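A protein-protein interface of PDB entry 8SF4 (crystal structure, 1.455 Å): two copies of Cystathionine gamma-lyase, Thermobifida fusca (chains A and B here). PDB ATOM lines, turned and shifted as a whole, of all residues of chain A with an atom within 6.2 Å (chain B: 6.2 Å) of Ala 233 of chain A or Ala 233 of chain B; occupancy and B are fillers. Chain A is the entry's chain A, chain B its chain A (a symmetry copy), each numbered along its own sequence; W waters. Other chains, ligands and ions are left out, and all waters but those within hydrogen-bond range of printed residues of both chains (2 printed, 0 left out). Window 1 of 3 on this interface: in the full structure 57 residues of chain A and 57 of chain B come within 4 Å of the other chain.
The side-chain hydroxyl of Ser 77 of chain A is in hydrogen-bond range of the backbone carbonyl oxygen of Gly 232 of chain B. N of Ala 80 of chain B sits close to O of Met 231 of chain A. The backbone carbonyl oxygen (O) of Gly 232 of chain A sits at hydrogen-bond distance from the side-chain hydroxyl (OG) of Ser 77 of chain B (2.7 Å). The backbone NH of Ala 80 of chain A lies close to the backbone carbonyl oxygen of Met 231 of chain B (3.1 Å). O of Met 231 of chain A lies close to O of Met 79 of chain B, at 3.5 Å.
The backbone carbonyl oxygen of Ala 80 of chain B is in hydrogen-bond range of the side-chain hydroxyl of Thr 84 of chain B (3.1 Å). The backbone carbonyl oxygen (O) of Ala 80 of chain A sits at hydrogen-bond distance from the side-chain hydroxyl (OG1) of Thr 84 of chain A, 3.1 Å away. NH2 of Arg 50 of chain B is in hydrogen-bond range of O of Asn 229 of chain B, 3.0 Å away. The guanidinium group of Arg 50 of chain A lies within hydrogen-bond range of the backbone carbonyl oxygen of Asn 229 of chain A (3.0 Å). The backbone NH (N) of Ala 76 of chain B sits at hydrogen-bond distance from the backbone carbonyl oxygen (O) of Ala 233 of chain B, 2.8 Å away. The backbone NH of Met 79 of chain B lies close to the side-chain hydroxyl of Ser 77 of chain B (3.4 Å).
CD of Arg 50 of chain A touches OG of Ser 77 of chain B, at 3.8 Å. Arg 50 of chain A touches Met 79 of chain B (NE to CG, 3.6 Å). Ala 76 of chain A touches Ala 76 of chain B (CB to CB, 3.9 Å). Gly 232 of chain B touches Ala 76 of chain A (O to CB, 3.7 Å). Arg 50 of chain B touches Ser 77 of chain A (CD to OG, 3.8 Å). Met 79 of chain A touches Met 231 of chain B (C to O, 3.4 Å). CB of Ala 80 of chain A touches O of Gly 232 of chain B (3.7 Å). Gly 232 of chain A touches Ala 76 of chain B (O to CB, 3.7 Å). CB of Ala 233 of chain A touches CB of Ala 233 of chain B, 3.6 Å away. O of Val 234 of chain A touches CB of Ala 76 of chain B (3.6 Å).
Of chain B, only Ala 233 (3.6 Å) comes within 4 Å of Ala 233 of chain A. Of the printed residues of chain B, Met 231 of chain A touches Met 79 (3.4 Å) and Ala 80 (3.1 Å). Of the printed residues of chain A, Arg 50 of chain B touches Ser 77 (3.8 Å) and Met 79 (3.6 Å). Printed residues of chain A within 4 Å of Ser 77 of chain B: Arg 50 and Gly 232. Thr 84 of chain B touches none of the printed residues of chain A. Ala 74 of chain B touches none of the printed residues of chain A. The nearest residue of chain B that does not touch Ala 233 of chain A is Ala 76 of chain B (4.1 Å). The nearest residue of chain A that does not touch Ala 233 of chain B is Ala 76 of chain A (4.1 Å). The nearest printed residue of chain A that does not touch Met 231 of chain B is Ser 77 of chain A (4.3 Å).
Of the 17 printed residues of chain B, 9 touch a printed residue of chain A. Printed residues of chain B that touch a printed residue of chain A: Arg 50, Ala 76, Ser 77, Met 79, Ala 80, Met 231, Gly 232, Ala 233 and Val 234. Among the printed residues, 18 pairs touch across the chains.
Ala 76 of chain A touches its own counterpart, Ala 76 of chain B. Ala 76 of chain A touches Val 234 of chain B, and with the chains exchanged Val 234 of chain A touches Ala 76 of chain B. Met 79 of chain A touches Met 231 of chain B, and with the chains exchanged Met 231 of chain A touches Met 79 of chain B. Ala 80 of chain A touches Gly 232 of chain B, and with the chains exchanged Gly 232 of chain A touches Ala 80 of chain B. Positions printed for both chains: 50, 74, 75, 76, 77, 79, 80, 81, 84, 227, 228, 229, 231, 232, 233, 234 and 235. Of the 18 pairs that touch across the chains among the printed residues, 18 have their exchanged pair printed and touching as well.
Water W1 lies within hydrogen-bond range of the backbone carbonyl oxygen (O) of Val 234 of chain A (2.8 Å) and the backbone carbonyl oxygen (O) of Ala 76 of chain B (2.9 Å). Water W2 lies within hydrogen-bond range of the backbone carbonyl oxygen of Val 234 of chain B (2.8 Å) and the backbone carbonyl oxygen of Ala 76 of chain A (2.9 Å).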
ATOM      1  N   ARG A  50     -20.049  29.250 -19.794  1.00  0.00           N
ATOM      2  CA  ARG A  50     -19.377  27.986 -19.348  1.00  0.00           C
ATOM      3  C   ARG A  50     -20.271  27.311 -18.307  1.00  0.00           C
ATOM      4  O   ARG A  50     -20.451  26.094 -18.361  1.00  0.00           O
ATOM      5  CB  ARG A  50     -17.999  28.318 -18.782  1.00  0.00           C
ATOM      6  CG  ARG A  50     -17.358  27.105 -18.128  1.00  0.00           C
ATOM      7  CD  ARG A  50     -15.882  27.288 -17.905  1.00  0.00           C
ATOM      8  NE  ARG A  50     -15.408  28.583 -17.512  1.00  0.00           N
ATOM      9  CZ  ARG A  50     -15.644  29.202 -16.376  1.00  0.00           C
ATOM     10  NH1 ARG A  50     -15.222  30.422 -16.173  1.00  0.00           N
ATOM     11  NH2 ARG A  50     -16.359  28.598 -15.438  1.00  0.00           N
ATOM     12  N   ALA A  74     -23.378  18.314 -21.451  1.00  0.00           N
ATOM     13  CA  ALA A  74     -22.683  18.290 -22.759  1.00  0.00           C
ATOM     14  C   ALA A  74     -21.286  18.846 -22.659  1.00  0.00           C
ATOM     15  O   ALA A  74     -21.036  19.888 -22.058  1.00  0.00           O
ATOM     16  CB  ALA A  74     -23.522  19.029 -23.798  1.00  0.00           C
ATOM     17  N   PHE A  75     -20.405  18.188 -23.406  1.00  0.00           N
ATOM     18  CA  PHE A  75     -18.957  18.420 -23.342  1.00  0.00           C
ATOM     19  C   PHE A  75     -18.341  18.624 -24.714  1.00  0.00           C
ATOM     20  O   PHE A  75     -18.931  18.249 -25.742  1.00  0.00           O
ATOM     21  CB  PHE A  75     -18.277  17.225 -22.602  1.00  0.00           C
ATOM     22  CG  PHE A  75     -18.703  17.115 -21.181  1.00  0.00           C
ATOM     23  CD1 PHE A  75     -19.800  16.380 -20.816  1.00  0.00           C
ATOM     24  CD2 PHE A  75     -18.017  17.797 -20.198  1.00  0.00           C
ATOM     25  CE1 PHE A  75     -20.231  16.346 -19.504  1.00  0.00           C
ATOM     26  CE2 PHE A  75     -18.447  17.789 -18.885  1.00  0.00           C
ATOM     27  CZ  PHE A  75     -19.550  17.036 -18.513  1.00  0.00           C
ATOM     28  N   ALA A  76     -17.111  19.083 -24.703  1.00  0.00           N
ATOM     29  CA  ALA A  76     -16.366  19.477 -25.910  1.00  0.00           C
ATOM     30  C   ALA A  76     -16.032  18.284 -26.823  1.00  0.00           C
ATOM     31  O   ALA A  76     -15.674  18.473 -28.003  1.00  0.00           O
ATOM     32  CB  ALA A  76     -15.047  20.096 -25.489  1.00  0.00           C
ATOM     33  N   SER A  77     -16.088  17.050 -26.305  1.00  0.00           N
ATOM     34  CA  SER A  77     -15.802  15.832 -27.023  1.00  0.00           C
ATOM     35  C   SER A  77     -16.263  14.684 -26.100  1.00  0.00           C
ATOM     36  O   SER A  77     -16.486  14.886 -24.894  1.00  0.00           O
ATOM     37  CB  SER A  77     -14.355  15.645 -27.344  1.00  0.00           C
ATOM     38  OG  SER A  77     -13.559  15.545 -26.118  1.00  0.00           O
ATOM     39  N   MET A  79     -14.259  12.326 -25.223  1.00  0.00           N
ATOM     40  CA  MET A  79     -13.144  12.198 -24.274  1.00  0.00           C
ATOM     41  C   MET A  79     -13.288  13.198 -23.108  1.00  0.00           C
ATOM     42  O   MET A  79     -12.961  12.834 -21.949  1.00  0.00           O
ATOM     43  CB  MET A  79     -11.814  12.267 -24.948  1.00  0.00           C
ATOM     44  CG  MET A  79     -11.472  11.089 -25.818  1.00  0.00           C
ATOM     45  SD  MET A  79     -11.725   9.469 -25.092  1.00  0.00           S
ATOM     46  CE  MET A  79     -10.944   9.676 -23.483  1.00  0.00           C
ATOM     47  N   ALA A  80     -13.755  14.394 -23.383  1.00  0.00           N
ATOM     48  CA  ALA A  80     -13.903  15.381 -22.301  1.00  0.00           C
ATOM     49  C   ALA A  80     -15.016  14.941 -21.349  1.00  0.00           C
ATOM     50  O   ALA A  80     -14.936  15.180 -20.105  1.00  0.00           O
ATOM     51  CB  ALA A  80     -14.190  16.749 -22.848  1.00  0.00           C
ATOM     52  N   ALA A  81     -16.086  14.323 -21.855  1.00  0.00           N
ATOM     53  CA  ALA A  81     -17.133  13.767 -20.989  1.00  0.00           C
ATOM     54  C   ALA A  81     -16.498  12.703 -20.064  1.00  0.00           C
ATOM     55  O   ALA A  81     -16.770  12.649 -18.866  1.00  0.00           O
ATOM     56  CB  ALA A  81     -18.251  13.183 -21.818  1.00  0.00           C
ATOM     57  N   THR A  84     -14.185  14.417 -17.414  1.00  0.00           N
ATOM     58  CA  THR A  84     -14.906  15.093 -16.338  1.00  0.00           C
ATOM     59  C   THR A  84     -15.555  14.072 -15.415  1.00  0.00           C
ATOM     60  O   THR A  84     -15.511  14.190 -14.209  1.00  0.00           O
ATOM     61  CB  THR A  84     -15.941  16.038 -16.944  1.00  0.00           C
ATOM     62  OG1 THR A  84     -15.210  17.050 -17.664  1.00  0.00           O
ATOM     63  CG2 THR A  84     -16.739  16.703 -15.912  1.00  0.00           C
ATOM     64  N   HIS A 227     -17.854  19.975 -11.963  1.00  0.00           N
ATOM     65  CA  HIS A 227     -16.636  19.767 -12.781  1.00  0.00           C
ATOM     66  C   HIS A 227     -16.811  20.291 -14.190  1.00  0.00           C
ATOM     67  O   HIS A 227     -15.831  20.726 -14.808  1.00  0.00           O
ATOM     68  CB  HIS A 227     -16.180  18.303 -12.670  1.00  0.00           C
ATOM     69  CG  HIS A 227     -15.631  17.935 -11.324  1.00  0.00           C
ATOM     70  ND1 HIS A 227     -16.448  17.680 -10.235  1.00  0.00           N
ATOM     71  CD2 HIS A 227     -14.359  17.835 -10.858  1.00  0.00           C
ATOM     72  CE1 HIS A 227     -15.677  17.493  -9.139  1.00  0.00           C
ATOM     73  NE2 HIS A 227     -14.411  17.495  -9.513  1.00  0.00           N
ATOM     74  N   GLN A 228     -17.974  20.147 -14.764  1.00  0.00           N
ATOM     75  CA  GLN A 228     -18.295  20.763 -16.066  1.00  0.00           C
ATOM     76  C   GLN A 228     -17.969  22.257 -15.982  1.00  0.00           C
ATOM     77  O   GLN A 228     -17.246  22.833 -16.851  1.00  0.00           O
ATOM     78  CB  GLN A 228     -19.763  20.568 -16.440  1.00  0.00           C
ATOM     79  CG  GLN A 228     -20.086  21.116 -17.858  1.00  0.00           C
ATOM     80  CD  GLN A 228     -21.578  21.119 -18.133  1.00  0.00           C
ATOM     81  OE1 GLN A 228     -22.337  21.553 -17.252  1.00  0.00           O
ATOM     82  NE2 GLN A 228     -22.008  20.694 -19.332  1.00  0.00           N
ATOM     83  N   ASN A 229     -18.454  22.966 -14.973  1.00  0.00           N
ATOM     84  CA  ASN A 229     -18.193  24.393 -14.804  1.00  0.00           C
ATOM     85  C   ASN A 229     -16.729  24.646 -14.475  1.00  0.00           C
ATOM     86  O   ASN A 229     -16.136  25.649 -14.981  1.00  0.00           O
ATOM     87  CB  ASN A 229     -19.144  24.998 -13.732  1.00  0.00           C
ATOM     88  CG  ASN A 229     -19.009  26.478 -13.593  1.00  0.00           C
ATOM     89  OD1 ASN A 229     -19.067  27.182 -14.595  1.00  0.00           O
ATOM     90  ND2 ASN A 229     -18.911  26.975 -12.359  1.00  0.00           N
ATOM     91  N   MET A 231     -13.766  22.754 -14.564  1.00  0.00           N
ATOM     92  CA  MET A 231     -12.766  22.303 -15.565  1.00  0.00           C
ATOM     93  C   MET A 231     -13.123  22.904 -16.930  1.00  0.00           C
ATOM     94  O   MET A 231     -12.210  23.024 -17.785  1.00  0.00           O
ATOM     95  CB  MET A 231     -12.697  20.782 -15.642  1.00  0.00           C
ATOM     96  CG  MET A 231     -12.167  20.195 -14.413  1.00  0.00           C
ATOM     97  SD  MET A 231     -12.528  18.409 -14.213  1.00  0.00           S
ATOM     98  CE  MET A 231     -12.236  17.815 -15.802  1.00  0.00           C
ATOM     99  N   GLY A 232     -14.365  23.216 -17.217  1.00  0.00           N
ATOM    100  CA  GLY A 232     -14.758  23.981 -18.397  1.00  0.00           C
ATOM    101  C   GLY A 232     -14.707  23.319 -19.717  1.00  0.00           C
ATOM    102  O   GLY A 232     -14.636  24.020 -20.732  1.00  0.00           O
ATOM    103  N   ALA A 233     -14.780  22.000 -19.791  1.00  0.00           N
ATOM    104  CA  ALA A 233     -14.668  21.304 -21.081  1.00  0.00           C
ATOM    105  C   ALA A 233     -16.017  21.174 -21.752  1.00  0.00           C
ATOM    106  O   ALA A 233     -16.494  20.070 -22.124  1.00  0.00           O
ATOM    107  CB  ALA A 233     -14.033  19.958 -20.858  1.00  0.00           C
ATOM    108  N   VAL A 234     -16.693  22.300 -21.935  1.00  0.00           N
ATOM    109  CA  VAL A 234     -18.091  22.370 -22.374  1.00  0.00           C
ATOM    110  C   VAL A 234     -18.189  22.294 -23.908  1.00  0.00           C
ATOM    111  O   VAL A 234     -17.293  22.690 -24.638  1.00  0.00           O
ATOM    112  CB  VAL A 234     -18.765  23.649 -21.876  1.00  0.00           C
ATOM    113  CG1 VAL A 234     -18.879  23.662 -20.347  1.00  0.00           C
ATOM    114  CG2 VAL A 234     -18.103  24.910 -22.404  1.00  0.00           C
ATOM    115  N   ALA A 235     -19.340  21.771 -24.360  1.00  0.00           N
ATOM    116  CA  ALA A 235     -19.769  21.923 -25.782  1.00  0.00           C
ATOM    117  C   ALA A 235     -20.103  23.395 -26.004  1.00  0.00           C
ATOM    118  O   ALA A 235     -20.911  23.960 -25.236  1.00  0.00           O
ATOM    119  CB  ALA A 235     -20.951  21.045 -26.081  1.00  0.00           C
ATOM    120  N   ARG B  50     -10.621  16.068 -32.980  1.00  0.00           N
ATOM    121  CA  ARG B  50     -10.144  16.305 -31.578  1.00  0.00           C
ATOM    122  C   ARG B  50      -8.620  16.417 -31.605  1.00  0.00           C
ATOM    123  O   ARG B  50      -8.065  17.300 -30.949  1.00  0.00           O
ATOM    124  CB  ARG B  50     -10.614  15.162 -30.683  1.00  0.00           C
ATOM    125  CG  ARG B  50      -9.988  15.243 -29.300  1.00  0.00           C
ATOM    126  CD  ARG B  50     -10.703  14.380 -28.297  1.00  0.00           C
ATOM    127  NE  ARG B  50     -11.200  13.105 -28.729  1.00  0.00           N
ATOM    128  CZ  ARG B  50     -10.490  12.063 -29.103  1.00  0.00           C
ATOM    129  NH1 ARG B  50     -11.068  10.982 -29.556  1.00  0.00           N
ATOM    130  NH2 ARG B  50      -9.167  12.124 -29.063  1.00  0.00           N
ATOM    131  N   ALA B  74      -5.569  25.465 -28.552  1.00  0.00           N
ATOM    132  CA  ALA B  74      -6.896  26.054 -28.261  1.00  0.00           C
ATOM    133  C   ALA B  74      -7.810  25.065 -27.583  1.00  0.00           C
ATOM    134  O   ALA B  74      -7.929  23.907 -27.974  1.00  0.00           O
ATOM    135  CB  ALA B  74      -7.504  26.606 -29.548  1.00  0.00           C
ATOM    136  N   PHE B  75      -8.568  25.614 -26.640  1.00  0.00           N
ATOM    137  CA  PHE B  75      -9.403  24.835 -25.718  1.00  0.00           C
ATOM    138  C   PHE B  75     -10.829  25.354 -25.646  1.00  0.00           C
ATOM    139  O   PHE B  75     -11.108  26.506 -26.018  1.00  0.00           O
ATOM    140  CB  PHE B  75      -8.743  24.833 -24.303  1.00  0.00           C
ATOM    141  CG  PHE B  75      -7.425  24.144 -24.288  1.00  0.00           C
ATOM    142  CD1 PHE B  75      -6.261  24.819 -24.545  1.00  0.00           C
ATOM    143  CD2 PHE B  75      -7.355  22.787 -24.055  1.00  0.00           C
ATOM    144  CE1 PHE B  75      -5.050  24.157 -24.604  1.00  0.00           C
ATOM    145  CE2 PHE B  75      -6.154  22.106 -24.129  1.00  0.00           C
ATOM    146  CZ  PHE B  75      -4.975  22.791 -24.378  1.00  0.00           C
ATOM    147  N   ALA B  76     -11.676  24.553 -25.043  1.00  0.00           N
ATOM    148  CA  ALA B  76     -13.127  24.790 -24.972  1.00  0.00           C
ATOM    149  C   ALA B  76     -13.493  26.011 -24.109  1.00  0.00           C
ATOM    150  O   ALA B  76     -14.630  26.518 -24.183  1.00  0.00           O
ATOM    151  CB  ALA B  76     -13.788  23.583 -24.334  1.00  0.00           C
ATOM    152  N   SER B  77     -12.579  26.479 -23.248  1.00  0.00           N
ATOM    153  CA  SER B  77     -12.765  27.607 -22.369  1.00  0.00           C
ATOM    154  C   SER B  77     -11.370  27.921 -21.789  1.00  0.00           C
ATOM    155  O   SER B  77     -10.446  27.092 -21.868  1.00  0.00           O
ATOM    156  CB  SER B  77     -13.711  27.346 -21.243  1.00  0.00           C
ATOM    157  OG  SER B  77     -13.204  26.283 -20.373  1.00  0.00           O
ATOM    158  N   MET B  79     -10.855  28.028 -18.615  1.00  0.00           N
ATOM    159  CA  MET B  79     -10.713  27.032 -17.543  1.00  0.00           C
ATOM    160  C   MET B  79     -10.187  25.692 -18.095  1.00  0.00           C
ATOM    161  O   MET B  79      -9.367  25.030 -17.408  1.00  0.00           O
ATOM    162  CB  MET B  79     -11.960  26.889 -16.734  1.00  0.00           C
ATOM    163  CG  MET B  79     -12.304  28.068 -15.867  1.00  0.00           C
ATOM    164  SD  MET B  79     -10.973  28.725 -14.861  1.00  0.00           S
ATOM    165  CE  MET B  79     -10.302  27.222 -14.134  1.00  0.00           C
ATOM    166  N   ALA B  80     -10.623  25.302 -19.271  1.00  0.00           N
ATOM    167  CA  ALA B  80     -10.151  24.025 -19.832  1.00  0.00           C
ATOM    168  C   ALA B  80      -8.668  24.134 -20.189  1.00  0.00           C
ATOM    169  O   ALA B  80      -7.895  23.135 -20.063  1.00  0.00           O
ATOM    170  CB  ALA B  80     -10.953  23.631 -21.037  1.00  0.00           C
ATOM    171  N   ALA B  81      -8.205  25.295 -20.660  1.00  0.00           N
ATOM    172  CA  ALA B  81      -6.774  25.508 -20.908  1.00  0.00           C
ATOM    173  C   ALA B  81      -6.007  25.319 -19.578  1.00  0.00           C
ATOM    174  O   ALA B  81      -4.958  24.679 -19.527  1.00  0.00           O
ATOM    175  CB  ALA B  81      -6.535  26.878 -21.494  1.00  0.00           C
ATOM    176  N   THR B  84      -6.020  21.549 -18.528  1.00  0.00           N
ATOM    177  CA  THR B  84      -5.114  20.708 -19.307  1.00  0.00           C
ATOM    178  C   THR B  84      -3.667  21.017 -18.948  1.00  0.00           C
ATOM    179  O   THR B  84      -2.855  20.134 -18.776  1.00  0.00           O
ATOM    180  CB  THR B  84      -5.381  20.927 -20.795  1.00  0.00           C
ATOM    181  OG1 THR B  84      -6.718  20.457 -21.051  1.00  0.00           O
ATOM    182  CG2 THR B  84      -4.460  20.152 -21.630  1.00  0.00           C
ATOM    183  N   HIS B 227      -2.290  15.939 -23.883  1.00  0.00           N
ATOM    184  CA  HIS B 227      -3.468  16.110 -23.000  1.00  0.00           C
ATOM    185  C   HIS B 227      -4.620  16.772 -23.726  1.00  0.00           C
ATOM    186  O   HIS B 227      -5.784  16.501 -23.403  1.00  0.00           O
ATOM    187  CB  HIS B 227      -3.038  16.783 -21.686  1.00  0.00           C
ATOM    188  CG  HIS B 227      -2.199  15.910 -20.801  1.00  0.00           C
ATOM    189  ND1 HIS B 227      -0.853  15.692 -21.037  1.00  0.00           N
ATOM    190  CD2 HIS B 227      -2.509  15.150 -19.718  1.00  0.00           C
ATOM    191  CE1 HIS B 227      -0.391  14.778 -20.152  1.00  0.00           C
ATOM    192  NE2 HIS B 227      -1.355  14.506 -19.291  1.00  0.00           N
ATOM    193  N   GLN B 228      -4.350  17.714 -24.587  1.00  0.00           N
ATOM    194  CA  GLN B 228      -5.381  18.307 -25.461  1.00  0.00           C
ATOM    195  C   GLN B 228      -6.106  17.168 -26.185  1.00  0.00           C
ATOM    196  O   GLN B 228      -7.372  17.077 -26.189  1.00  0.00           O
ATOM    197  CB  GLN B 228      -4.778  19.274 -26.477  1.00  0.00           C
ATOM    198  CG  GLN B 228      -5.866  19.986 -27.327  1.00  0.00           C
ATOM    199  CD  GLN B 228      -5.257  20.773 -28.473  1.00  0.00           C
ATOM    200  OE1 GLN B 228      -4.375  20.228 -29.156  1.00  0.00           O
ATOM    201  NE2 GLN B 228      -5.730  22.004 -28.726  1.00  0.00           N
ATOM    202  N   ASN B 229      -5.391  16.253 -26.825  1.00  0.00           N
ATOM    203  CA  ASN B 229      -5.991  15.130 -27.538  1.00  0.00           C
ATOM    204  C   ASN B 229      -6.649  14.156 -26.571  1.00  0.00           C
ATOM    205  O   ASN B 229      -7.751  13.609 -26.884  1.00  0.00           O
ATOM    206  CB  ASN B 229      -4.933  14.429 -28.439  1.00  0.00           C
ATOM    207  CG  ASN B 229      -5.509  13.343 -29.285  1.00  0.00           C
ATOM    208  OD1 ASN B 229      -6.499  13.575 -29.970  1.00  0.00           O
ATOM    209  ND2 ASN B 229      -4.859  12.178 -29.318  1.00  0.00           N
ATOM    210  N   MET B 231      -7.555  14.210 -23.173  1.00  0.00           N
ATOM    211  CA  MET B 231      -8.649  14.745 -22.324  1.00  0.00           C
ATOM    212  C   MET B 231      -9.701  15.403 -23.225  1.00  0.00           C
ATOM    213  O   MET B 231     -10.873  15.515 -22.788  1.00  0.00           O
ATOM    214  CB  MET B 231      -8.123  15.734 -21.291  1.00  0.00           C
ATOM    215  CG  MET B 231      -7.270  15.086 -20.296  1.00  0.00           C
ATOM    216  SD  MET B 231      -6.199  16.237 -19.354  1.00  0.00           S
ATOM    217  CE  MET B 231      -7.282  17.538 -19.037  1.00  0.00           C
ATOM    218  N   GLY B 232      -9.363  15.899 -24.392  1.00  0.00           N
ATOM    219  CA  GLY B 232     -10.326  16.347 -25.394  1.00  0.00           C
ATOM    220  C   GLY B 232     -11.053  17.611 -25.160  1.00  0.00           C
ATOM    221  O   GLY B 232     -12.122  17.802 -25.750  1.00  0.00           O
ATOM    222  N   ALA B 233     -10.530  18.528 -24.363  1.00  0.00           N
ATOM    223  CA  ALA B 233     -11.253  19.771 -24.055  1.00  0.00           C
ATOM    224  C   ALA B 233     -10.959  20.843 -25.081  1.00  0.00           C
ATOM    225  O   ALA B 233     -10.523  21.984 -24.774  1.00  0.00           O
ATOM    226  CB  ALA B 233     -10.887  20.221 -22.668  1.00  0.00           C
ATOM    227  N   VAL B 234     -11.185  20.523 -26.347  1.00  0.00           N
ATOM    228  CA  VAL B 234     -10.775  21.336 -27.498  1.00  0.00           C
ATOM    229  C   VAL B 234     -11.816  22.430 -27.795  1.00  0.00           C
ATOM    230  O   VAL B 234     -13.000  22.291 -27.529  1.00  0.00           O
ATOM    231  CB  VAL B 234     -10.564  20.471 -28.741  1.00  0.00           C
ATOM    232  CG1 VAL B 234      -9.386  19.507 -28.559  1.00  0.00           C
ATOM    233  CG2 VAL B 234     -11.826  19.746 -29.177  1.00  0.00           C
ATOM    234  N   ALA B 235     -11.308  23.527 -28.378  1.00  0.00           N
ATOM    235  CA  ALA B 235     -12.180  24.538 -29.048  1.00  0.00           C
ATOM    236  C   ALA B 235     -12.761  23.883 -30.298  1.00  0.00           C
ATOM    237  O   ALA B 235     -11.989  23.350 -31.123  1.00  0.00           O
ATOM    238  CB  ALA B 235     -11.399  25.774 -29.393  1.00  0.00           C
HETATM  239  O   HOH W   1     -16.447  25.091 -25.894  1.00  0.00           O
HETATM  240  O   HOH W   2     -15.360  21.242 -28.708  1.00  0.00           O
